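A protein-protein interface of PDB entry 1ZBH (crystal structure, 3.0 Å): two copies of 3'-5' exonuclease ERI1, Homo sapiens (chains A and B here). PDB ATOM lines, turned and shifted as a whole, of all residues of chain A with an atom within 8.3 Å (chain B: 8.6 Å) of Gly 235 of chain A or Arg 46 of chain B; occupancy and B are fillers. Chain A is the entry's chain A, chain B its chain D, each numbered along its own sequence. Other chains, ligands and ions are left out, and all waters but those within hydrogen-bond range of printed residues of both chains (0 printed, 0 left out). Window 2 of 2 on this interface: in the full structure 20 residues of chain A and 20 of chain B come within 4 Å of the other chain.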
ATOM      1  N   TYR A 214      -8.059   9.156  23.322  1.00  0.00           N
ATOM      2  CA  TYR A 214      -8.093   9.150  21.860  1.00  0.00           C
ATOM      3  C   TYR A 214      -6.870   9.871  21.295  1.00  0.00           C
ATOM      4  O   TYR A 214      -6.160   9.330  20.445  1.00  0.00           O
ATOM      5  CB  TYR A 214      -9.380   9.824  21.377  1.00  0.00           C
ATOM      6  CG  TYR A 214      -9.763   9.586  19.931  1.00  0.00           C
ATOM      7  CD1 TYR A 214     -10.670   8.581  19.588  1.00  0.00           C
ATOM      8  CD2 TYR A 214      -9.255  10.392  18.912  1.00  0.00           C
ATOM      9  CE1 TYR A 214     -11.042   8.371  18.266  1.00  0.00           C
ATOM     10  CE2 TYR A 214      -9.618  10.189  17.589  1.00  0.00           C
ATOM     11  CZ  TYR A 214     -10.511   9.180  17.273  1.00  0.00           C
ATOM     12  OH  TYR A 214     -10.870   8.983  15.962  1.00  0.00           O
ATOM     13  N   THR A 228     -18.058  14.369  17.379  1.00  0.00           N
ATOM     14  CA  THR A 228     -18.389  14.130  15.968  1.00  0.00           C
ATOM     15  C   THR A 228     -17.146  13.907  15.110  1.00  0.00           C
ATOM     16  O   THR A 228     -17.206  13.186  14.115  1.00  0.00           O
ATOM     17  CB  THR A 228     -19.252  15.262  15.338  1.00  0.00           C
ATOM     18  OG1 THR A 228     -18.478  16.462  15.222  1.00  0.00           O
ATOM     19  CG2 THR A 228     -20.508  15.532  16.171  1.00  0.00           C
ATOM     20  N   ILE A 229     -16.030  14.522  15.495  1.00  0.00           N
ATOM     21  CA  ILE A 229     -14.776  14.367  14.752  1.00  0.00           C
ATOM     22  C   ILE A 229     -14.105  13.028  15.070  1.00  0.00           C
ATOM     23  O   ILE A 229     -13.597  12.359  14.167  1.00  0.00           O
ATOM     24  CB  ILE A 229     -13.792  15.552  14.968  1.00  0.00           C
ATOM     25  CG1 ILE A 229     -14.502  16.892  14.747  1.00  0.00           C
ATOM     26  CG2 ILE A 229     -12.599  15.443  14.017  1.00  0.00           C
ATOM     27  CD1 ILE A 229     -13.714  18.112  15.217  1.00  0.00           C
ATOM     28  N   MET A 230     -14.116  12.634  16.342  1.00  0.00           N
ATOM     29  CA  MET A 230     -13.576  11.333  16.747  1.00  0.00           C
ATOM     30  C   MET A 230     -14.265  10.199  15.997  1.00  0.00           C
ATOM     31  O   MET A 230     -13.607   9.267  15.529  1.00  0.00           O
ATOM     32  CB  MET A 230     -13.711  11.123  18.256  1.00  0.00           C
ATOM     33  CG  MET A 230     -12.683  11.879  19.082  1.00  0.00           C
ATOM     34  SD  MET A 230     -12.693  11.421  20.826  1.00  0.00           S
ATOM     35  CE  MET A 230     -14.244  12.122  21.376  1.00  0.00           C
ATOM     36  N   LEU A 231     -15.589  10.296  15.883  1.00  0.00           N
ATOM     37  CA  LEU A 231     -16.381   9.343  15.113  1.00  0.00           C
ATOM     38  C   LEU A 231     -15.959   9.348  13.650  1.00  0.00           C
ATOM     39  O   LEU A 231     -15.663   8.296  13.084  1.00  0.00           O
ATOM     40  CB  LEU A 231     -17.873   9.673  15.219  1.00  0.00           C
ATOM     41  CG  LEU A 231     -18.611   9.421  16.535  1.00  0.00           C
ATOM     42  CD1 LEU A 231     -19.933  10.161  16.521  1.00  0.00           C
ATOM     43  CD2 LEU A 231     -18.827   7.934  16.779  1.00  0.00           C
ATOM     44  N   GLU A 232     -15.921  10.537  13.051  1.00  0.00           N
ATOM     45  CA  GLU A 232     -15.579  10.689  11.638  1.00  0.00           C
ATOM     46  C   GLU A 232     -14.214  10.080  11.317  1.00  0.00           C
ATOM     47  O   GLU A 232     -14.077   9.349  10.338  1.00  0.00           O
ATOM     48  CB  GLU A 232     -15.621  12.162  11.220  1.00  0.00           C
ATOM     49  CG  GLU A 232     -15.708  12.363   9.706  1.00  0.00           C
ATOM     50  CD  GLU A 232     -15.163  13.709   9.232  1.00  0.00           C
ATOM     51  OE1 GLU A 232     -14.802  13.808   8.039  1.00  0.00           O
ATOM     52  OE2 GLU A 232     -15.092  14.663  10.042  1.00  0.00           O
ATOM     53  N   LYS A 233     -13.221  10.368  12.159  1.00  0.00           N
ATOM     54  CA  LYS A 233     -11.860   9.853  11.982  1.00  0.00           C
ATOM     55  C   LYS A 233     -11.773   8.335  12.128  1.00  0.00           C
ATOM     56  O   LYS A 233     -10.804   7.719  11.684  1.00  0.00           O
ATOM     57  CB  LYS A 233     -10.884  10.540  12.944  1.00  0.00           C
ATOM     58  CG  LYS A 233     -10.698  12.023  12.661  1.00  0.00           C
ATOM     59  CD  LYS A 233      -9.365  12.545  13.156  1.00  0.00           C
ATOM     60  CE  LYS A 233      -9.117  13.942  12.611  1.00  0.00           C
ATOM     61  NZ  LYS A 233      -7.696  14.360  12.736  1.00  0.00           N
ATOM     62  N   LEU A 234     -12.791   7.744  12.750  1.00  0.00           N
ATOM     63  CA  LEU A 234     -12.899   6.291  12.872  1.00  0.00           C
ATOM     64  C   LEU A 234     -13.769   5.699  11.765  1.00  0.00           C
ATOM     65  O   LEU A 234     -14.066   4.502  11.773  1.00  0.00           O
ATOM     66  CB  LEU A 234     -13.444   5.897  14.248  1.00  0.00           C
ATOM     67  CG  LEU A 234     -12.542   6.110  15.467  1.00  0.00           C
ATOM     68  CD1 LEU A 234     -13.307   5.807  16.741  1.00  0.00           C
ATOM     69  CD2 LEU A 234     -11.277   5.265  15.386  1.00  0.00           C
ATOM     70  N   GLY A 235     -14.172   6.549  10.823  1.00  0.00           N
ATOM     71  CA  GLY A 235     -14.925   6.125   9.645  1.00  0.00           C
ATOM     72  C   GLY A 235     -16.369   5.759   9.925  1.00  0.00           C
ATOM     73  O   GLY A 235     -16.939   4.896   9.255  1.00  0.00           O
ATOM     74  N   MET A 236     -16.963   6.423  10.913  1.00  0.00           N
ATOM     75  CA  MET A 236     -18.343   6.148  11.315  1.00  0.00           C
ATOM     76  C   MET A 236     -19.131   7.435  11.582  1.00  0.00           C
ATOM     77  O   MET A 236     -18.562   8.452  11.990  1.00  0.00           O
ATOM     78  CB  MET A 236     -18.378   5.202  12.528  1.00  0.00           C
ATOM     79  CG  MET A 236     -17.571   5.673  13.744  1.00  0.00           C
ATOM     80  SD  MET A 236     -16.925   4.345  14.794  1.00  0.00           S
ATOM     81  CE  MET A 236     -18.422   3.698  15.532  1.00  0.00           C
ATOM     82  N   ASP A 237     -20.438   7.381  11.337  1.00  0.00           N
ATOM     83  CA  ASP A 237     -21.315   8.530  11.552  1.00  0.00           C
ATOM     84  C   ASP A 237     -22.008   8.466  12.909  1.00  0.00           C
ATOM     85  O   ASP A 237     -21.923   7.456  13.609  1.00  0.00           O
ATOM     86  CB  ASP A 237     -22.344   8.629  10.424  1.00  0.00           C
ATOM     87  CG  ASP A 237     -21.718   9.020   9.105  1.00  0.00           C
ATOM     88  OD1 ASP A 237     -21.354  10.205   8.941  1.00  0.00           O
ATOM     89  OD2 ASP A 237     -21.592   8.141   8.228  1.00  0.00           O
ATOM     90  N   TYR A 238     -22.687   9.552  13.271  1.00  0.00           N
ATOM     91  CA  TYR A 238     -23.395   9.643  14.543  1.00  0.00           C
ATOM     92  C   TYR A 238     -24.715   8.871  14.507  1.00  0.00           C
ATOM     93  O   TYR A 238     -25.523   9.048  13.589  1.00  0.00           O
ATOM     94  CB  TYR A 238     -23.651  11.111  14.898  1.00  0.00           C
ATOM     95  CG  TYR A 238     -24.107  11.341  16.321  1.00  0.00           C
ATOM     96  CD1 TYR A 238     -23.193  11.675  17.321  1.00  0.00           C
ATOM     97  CD2 TYR A 238     -25.453  11.238  16.668  1.00  0.00           C
ATOM     98  CE1 TYR A 238     -23.607  11.891  18.634  1.00  0.00           C
ATOM     99  CE2 TYR A 238     -25.876  11.447  17.975  1.00  0.00           C
ATOM    100  CZ  TYR A 238     -24.951  11.777  18.953  1.00  0.00           C
ATOM    101  OH  TYR A 238     -25.373  11.988  20.246  1.00  0.00           O
ATOM    102  N   ARG A 254     -19.330   3.629  21.270  1.00  0.00           N
ATOM    103  CA  ARG A 254     -18.904   3.122  19.966  1.00  0.00           C
ATOM    104  C   ARG A 254     -17.422   3.397  19.719  1.00  0.00           C
ATOM    105  O   ARG A 254     -16.715   2.552  19.168  1.00  0.00           O
ATOM    106  CB  ARG A 254     -19.748   3.730  18.843  1.00  0.00           C
ATOM    107  CG  ARG A 254     -21.184   3.240  18.801  1.00  0.00           C
ATOM    108  CD  ARG A 254     -21.993   4.027  17.792  1.00  0.00           C
ATOM    109  NE  ARG A 254     -21.667   3.645  16.422  1.00  0.00           N
ATOM    110  CZ  ARG A 254     -21.887   4.407  15.355  1.00  0.00           C
ATOM    111  NH1 ARG A 254     -22.431   5.611  15.488  1.00  0.00           N
ATOM    112  NH2 ARG A 254     -21.556   3.965  14.150  1.00  0.00           N
ATOM    113  N   ARG A 258     -14.269   0.543  19.569  1.00  0.00           N
ATOM    114  CA  ARG A 258     -13.301   0.637  18.478  1.00  0.00           C
ATOM    115  C   ARG A 258     -11.870   0.742  18.999  1.00  0.00           C
ATOM    116  O   ARG A 258     -10.966   0.084  18.486  1.00  0.00           O
ATOM    117  CB  ARG A 258     -13.640   1.832  17.578  1.00  0.00           C
ATOM    118  CG  ARG A 258     -12.746   2.007  16.354  1.00  0.00           C
ATOM    119  CD  ARG A 258     -13.122   1.061  15.225  1.00  0.00           C
ATOM    120  NE  ARG A 258     -12.459  -0.235  15.344  1.00  0.00           N
ATOM    121  CZ  ARG A 258     -12.858  -1.342  14.726  1.00  0.00           C
ATOM    122  NH1 ARG A 258     -13.933  -1.326  13.948  1.00  0.00           N
ATOM    123  NH2 ARG A 258     -12.188  -2.473  14.896  1.00  0.00           N
ATOM    124  N   ASP A 262      -8.734  -1.937  18.875  1.00  0.00           N
ATOM    125  CA  ASP A 262      -7.440  -1.571  18.307  1.00  0.00           C
ATOM    126  C   ASP A 262      -6.298  -1.748  19.303  1.00  0.00           C
ATOM    127  O   ASP A 262      -5.134  -1.494  18.980  1.00  0.00           O
ATOM    128  CB  ASP A 262      -7.479  -0.136  17.778  1.00  0.00           C
ATOM    129  CG  ASP A 262      -8.416   0.023  16.598  1.00  0.00           C
ATOM    130  OD1 ASP A 262      -8.946  -0.994  16.103  1.00  0.00           O
ATOM    131  OD2 ASP A 262      -8.623   1.174  16.163  1.00  0.00           O
ATOM    132  N   LYS B  31      -1.424   5.047   3.190  1.00  0.00           N
ATOM    133  CA  LYS B  31      -2.846   4.747   3.415  1.00  0.00           C
ATOM    134  C   LYS B  31      -3.277   3.471   2.692  1.00  0.00           C
ATOM    135  O   LYS B  31      -3.997   2.644   3.257  1.00  0.00           O
ATOM    136  CB  LYS B  31      -3.728   5.919   2.957  1.00  0.00           C
ATOM    137  CG  LYS B  31      -5.175   5.911   3.481  1.00  0.00           C
ATOM    138  CD  LYS B  31      -5.356   6.901   4.633  1.00  0.00           C
ATOM    139  CE  LYS B  31      -6.794   7.424   4.729  1.00  0.00           C
ATOM    140  NZ  LYS B  31      -6.876   8.707   5.509  1.00  0.00           N
ATOM    141  N   LEU B  34      -1.397   0.315   4.092  1.00  0.00           N
ATOM    142  CA  LEU B  34      -2.035   0.007   5.370  1.00  0.00           C
ATOM    143  C   LEU B  34      -3.382  -0.677   5.162  1.00  0.00           C
ATOM    144  O   LEU B  34      -3.646  -1.709   5.774  1.00  0.00           O
ATOM    145  CB  LEU B  34      -2.194   1.269   6.227  1.00  0.00           C
ATOM    146  CG  LEU B  34      -0.924   1.943   6.760  1.00  0.00           C
ATOM    147  CD1 LEU B  34      -1.233   3.359   7.205  1.00  0.00           C
ATOM    148  CD2 LEU B  34      -0.285   1.154   7.894  1.00  0.00           C
ATOM    149  N   ARG B  35      -4.218  -0.108   4.291  1.00  0.00           N
ATOM    150  CA  ARG B  35      -5.509  -0.712   3.940  1.00  0.00           C
ATOM    151  C   ARG B  35      -5.355  -2.099   3.322  1.00  0.00           C
ATOM    152  O   ARG B  35      -6.185  -2.980   3.553  1.00  0.00           O
ATOM    153  CB  ARG B  35      -6.311   0.191   3.000  1.00  0.00           C
ATOM    154  CG  ARG B  35      -7.291   1.097   3.717  1.00  0.00           C
ATOM    155  CD  ARG B  35      -8.430   1.539   2.812  1.00  0.00           C
ATOM    156  NE  ARG B  35      -8.061   2.673   1.966  1.00  0.00           N
ATOM    157  CZ  ARG B  35      -8.154   3.952   2.327  1.00  0.00           C
ATOM    158  NH1 ARG B  35      -8.601   4.283   3.534  1.00  0.00           N
ATOM    159  NH2 ARG B  35      -7.795   4.908   1.477  1.00  0.00           N
ATOM    160  N   LEU B  38      -4.120  -4.649   5.969  1.00  0.00           N
ATOM    161  CA  LEU B  38      -5.198  -4.747   6.950  1.00  0.00           C
ATOM    162  C   LEU B  38      -6.285  -5.713   6.478  1.00  0.00           C
ATOM    163  O   LEU B  38      -6.771  -6.529   7.265  1.00  0.00           O
ATOM    164  CB  LEU B  38      -5.784  -3.360   7.243  1.00  0.00           C
ATOM    165  CG  LEU B  38      -6.025  -2.915   8.692  1.00  0.00           C
ATOM    166  CD1 LEU B  38      -4.885  -3.310   9.616  1.00  0.00           C
ATOM    167  CD2 LEU B  38      -6.232  -1.408   8.744  1.00  0.00           C
ATOM    168  N   SER B  39      -6.654  -5.624   5.197  1.00  0.00           N
ATOM    169  CA  SER B  39      -7.595  -6.567   4.574  1.00  0.00           C
ATOM    170  C   SER B  39      -7.042  -7.989   4.610  1.00  0.00           C
ATOM    171  O   SER B  39      -7.793  -8.960   4.733  1.00  0.00           O
ATOM    172  CB  SER B  39      -7.881  -6.173   3.123  1.00  0.00           C
ATOM    173  OG  SER B  39      -8.758  -5.065   3.045  1.00  0.00           O
ATOM    174  N   LEU B  43      -8.717  -7.484   9.555  1.00  0.00           N
ATOM    175  CA  LEU B  43      -8.929  -6.370  10.475  1.00  0.00           C
ATOM    176  C   LEU B  43      -9.707  -5.263   9.771  1.00  0.00           C
ATOM    177  O   LEU B  43      -9.751  -5.221   8.538  1.00  0.00           O
ATOM    178  CB  LEU B  43      -7.586  -5.846  10.996  1.00  0.00           C
ATOM    179  CG  LEU B  43      -6.668  -6.860  11.691  1.00  0.00           C
ATOM    180  CD1 LEU B  43      -5.236  -6.355  11.761  1.00  0.00           C
ATOM    181  CD2 LEU B  43      -7.176  -7.229  13.081  1.00  0.00           C
ATOM    182  N   GLU B  44     -10.324  -4.377  10.551  1.00  0.00           N
ATOM    183  CA  GLU B  44     -11.163  -3.314   9.996  1.00  0.00           C
ATOM    184  C   GLU B  44     -10.312  -2.357   9.172  1.00  0.00           C
ATOM    185  O   GLU B  44      -9.213  -1.992   9.586  1.00  0.00           O
ATOM    186  CB  GLU B  44     -11.888  -2.553  11.110  1.00  0.00           C
ATOM    187  CG  GLU B  44     -13.415  -2.505  10.956  1.00  0.00           C
ATOM    188  CD  GLU B  44     -13.909  -1.505   9.918  1.00  0.00           C
ATOM    189  OE1 GLU B  44     -15.139  -1.307   9.835  1.00  0.00           O
ATOM    190  OE2 GLU B  44     -13.085  -0.918   9.189  1.00  0.00           O
ATOM    191  N   THR B  45     -10.824  -1.960   8.009  1.00  0.00           N
ATOM    192  CA  THR B  45     -10.062  -1.134   7.066  1.00  0.00           C
ATOM    193  C   THR B  45     -10.507   0.328   7.009  1.00  0.00           C
ATOM    194  O   THR B  45      -9.755   1.188   6.535  1.00  0.00           O
ATOM    195  CB  THR B  45     -10.083  -1.727   5.641  1.00  0.00           C
ATOM    196  OG1 THR B  45     -11.438  -1.945   5.231  1.00  0.00           O
ATOM    197  CG2 THR B  45      -9.318  -3.045   5.600  1.00  0.00           C
ATOM    198  N   ARG B  46     -11.722   0.603   7.485  1.00  0.00           N
ATOM    199  CA  ARG B  46     -12.247   1.969   7.546  1.00  0.00           C
ATOM    200  C   ARG B  46     -11.475   2.814   8.557  1.00  0.00           C
ATOM    201  O   ARG B  46     -10.957   2.292   9.551  1.00  0.00           O
ATOM    202  CB  ARG B  46     -13.739   1.974   7.900  1.00  0.00           C
ATOM    203  CG  ARG B  46     -14.641   1.287   6.880  1.00  0.00           C
ATOM    204  CD  ARG B  46     -16.089   1.760   6.984  1.00  0.00           C
ATOM    205  NE  ARG B  46     -16.239   3.160   6.577  1.00  0.00           N
ATOM    206  CZ  ARG B  46     -17.389   3.734   6.225  1.00  0.00           C
ATOM    207  NH1 ARG B  46     -18.523   3.036   6.216  1.00  0.00           N
ATOM    208  NH2 ARG B  46     -17.406   5.014   5.874  1.00  0.00           N
ATOM    209  N   GLY B  47     -11.398   4.117   8.290  1.00  0.00           N
ATOM    210  CA  GLY B  47     -10.758   5.061   9.204  1.00  0.00           C
ATOM    211  C   GLY B  47      -9.929   6.135   8.525  1.00  0.00           C
ATOM    212  O   GLY B  47     -10.281   6.625   7.448  1.00  0.00           O
ATOM    213  N   VAL B  48      -8.831   6.508   9.181  1.00  0.00           N
ATOM    214  CA  VAL B  48      -7.895   7.521   8.690  1.00  0.00           C
ATOM    215  C   VAL B  48      -6.473   6.961   8.808  1.00  0.00           C
ATOM    216  O   VAL B  48      -6.240   6.001   9.543  1.00  0.00           O
ATOM    217  CB  VAL B  48      -8.054   8.867   9.471  1.00  0.00           C
ATOM    218  CG1 VAL B  48      -6.855   9.794   9.272  1.00  0.00           C
ATOM    219  CG2 VAL B  48      -9.340   9.576   9.062  1.00  0.00           C
ATOM    220  N   LYS B  49      -5.539   7.558   8.070  1.00  0.00           N
ATOM    221  CA  LYS B  49      -4.120   7.185   8.097  1.00  0.00           C
ATOM    222  C   LYS B  49      -3.605   6.777   9.484  1.00  0.00           C
ATOM    223  O   LYS B  49      -3.056   5.686   9.647  1.00  0.00           O
ATOM    224  CB  LYS B  49      -3.272   8.333   7.532  1.00  0.00           C
ATOM    225  CG  LYS B  49      -1.767   8.079   7.522  1.00  0.00           C
ATOM    226  CD  LYS B  49      -0.993   9.361   7.214  1.00  0.00           C
ATOM    227  CE  LYS B  49       0.501   9.097   7.030  1.00  0.00           C
ATOM    228  NZ  LYS B  49       0.790   8.202   5.866  1.00  0.00           N
ATOM    229  N   VAL B  51      -5.224   6.134  12.282  1.00  0.00           N
ATOM    230  CA  VAL B  51      -6.021   5.076  12.905  1.00  0.00           C
ATOM    231  C   VAL B  51      -5.563   3.699  12.408  1.00  0.00           C
ATOM    232  O   VAL B  51      -5.206   2.823  13.204  1.00  0.00           O
ATOM    233  CB  VAL B  51      -7.526   5.274  12.619  1.00  0.00           C
ATOM    234  CG1 VAL B  51      -8.345   4.149  13.223  1.00  0.00           C
ATOM    235  CG2 VAL B  51      -7.997   6.616  13.152  1.00  0.00           C
ATOM    236  N   LEU B  52      -5.576   3.534  11.084  1.00  0.00           N
ATOM    237  CA  LEU B  52      -5.061   2.349  10.399  1.00  0.00           C
ATOM    238  C   LEU B  52      -3.617   2.045  10.795  1.00  0.00           C
ATOM    239  O   LEU B  52      -3.236   0.882  10.930  1.00  0.00           O
ATOM    240  CB  LEU B  52      -5.131   2.561   8.885  1.00  0.00           C
ATOM    241  CG  LEU B  52      -6.431   2.406   8.091  1.00  0.00           C
ATOM    242  CD1 LEU B  52      -7.642   3.087   8.724  1.00  0.00           C
ATOM    243  CD2 LEU B  52      -6.200   2.946   6.694  1.00  0.00           C
ATOM    244  N   LYS B  53      -2.824   3.097  10.975  1.00  0.00           N
ATOM    245  CA  LYS B  53      -1.431   2.963  11.381  1.00  0.00           C
ATOM    246  C   LYS B  53      -1.311   2.338  12.776  1.00  0.00           C
ATOM    247  O   LYS B  53      -0.540   1.400  12.969  1.00  0.00           O
ATOM    248  CB  LYS B  53      -0.724   4.322  11.324  1.00  0.00           C
ATOM    249  CG  LYS B  53       0.797   4.248  11.349  1.00  0.00           C
ATOM    250  CD  LYS B  53       1.446   5.582  10.964  1.00  0.00           C
ATOM    251  CE  LYS B  53       1.546   5.763   9.445  1.00  0.00           C
ATOM    252  NZ  LYS B  53       2.318   6.985   9.077  1.00  0.00           N
ATOM    253  N   ARG B  55      -3.694   0.692  14.465  1.00  0.00           N
ATOM    254  CA  ARG B  55      -4.364  -0.606  14.446  1.00  0.00           C
ATOM    255  C   ARG B  55      -3.415  -1.719  13.996  1.00  0.00           C
ATOM    256  O   ARG B  55      -3.295  -2.751  14.659  1.00  0.00           O
ATOM    257  CB  ARG B  55      -5.583  -0.543  13.525  1.00  0.00           C
ATOM    258  CG  ARG B  55      -6.513  -1.745  13.597  1.00  0.00           C
ATOM    259  CD  ARG B  55      -7.779  -1.486  12.796  1.00  0.00           C
ATOM    260  NE  ARG B  55      -8.585  -0.411  13.377  1.00  0.00           N
ATOM    261  CZ  ARG B  55      -9.443   0.348  12.700  1.00  0.00           C
ATOM    262  NH1 ARG B  55      -9.624   0.173  11.397  1.00  0.00           N
ATOM    263  NH2 ARG B  55     -10.124   1.292  13.330  1.00  0.00           N
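The backbone NH (N) of Val 48 of chain B sits at hydrogen-bond distance from the backbone carbonyl oxygen (O) of Lys 233 of chain A (3.4 Å).
The backbone carbonyl oxygen of Gly 235 of chain A sits at hydrogen-bond distance from the guanidinium group of Arg 46 of chain B, at 3.3 Å.
The side-chain carboxylate (OD1) of Asp 262 of chain A lies within salt-bridge range of the guanidinium group (NE) of Arg 55 of chain B.
The guanidinium group (NH2) of Arg 55 of chain B lies close to the guanidinium group (NE) of Arg 258 of chain A (3.4 Å).
NE of Arg 258 of chain A lies within salt-bridge range of OD1 of Asp 262 of chain A (3.7 Å).
OE2 of Glu 44 of chain B is in hydrogen-bond range of N of Arg 46 of chain B (2.7 Å).
NH1 of Arg 55 of chain B is in hydrogen-bond range of O of Glu 44 of chain B.
O of Arg 46 of chain B is in hydrogen-bond range of NH1 of Arg 55 of chain B (3.1 Å).
Gly 47 of chain B touches Lys 233 of chain A (CA to O, 3.6 Å).
Lys 233 of chain A touches Val 51 of chain B (O to CG2, 3.4 Å).
Leu 234 of chain A touches Val 51 of chain B (CD2 to CG1, 3.8 Å).
NH1 of Arg 258 of chain A touches CG of Glu 44 of chain B, 3.3 Å away.
Arg 46 of chain B touches just one residue of chain A: Gly 235 (3.3 Å).
Of the printed residues of chain A, Glu 44 of chain B touches Arg 258.
Of the printed residues of chain A, Gly 47 of chain B touches Lys 233.
Of the printed residues of chain B, Arg 258 of chain A touches Glu 44 (3.3 Å) and Arg 55 (3.4 Å).
The nearest printed residue of chain A that does not touch Gly 47 of chain B is Leu 234 of chain A (4.004 Å).
Printed residues of chain B that touch a printed residue of chain A: Glu 44, Arg 46, Gly 47, Val 48, Val 51 and Arg 55.
Hydrophobic or aromatic side chains of chain B within 4 Å of the printed part of chain A: Val 48 and Val 51.
Along chain B the printed residues that touch a printed residue of chain A span positions 44 to 55.
Of the 15 printed residues of chain A, 5 touch a printed residue of chain B.
Hydrophobic or aromatic side chains of chain A within 4 Å of the printed part of chain B: Leu 234.
No position is printed for both chains.
Of the 8 pairs that touch across the chains among the printed residues, none has its exchanged pair printed and touching as well.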
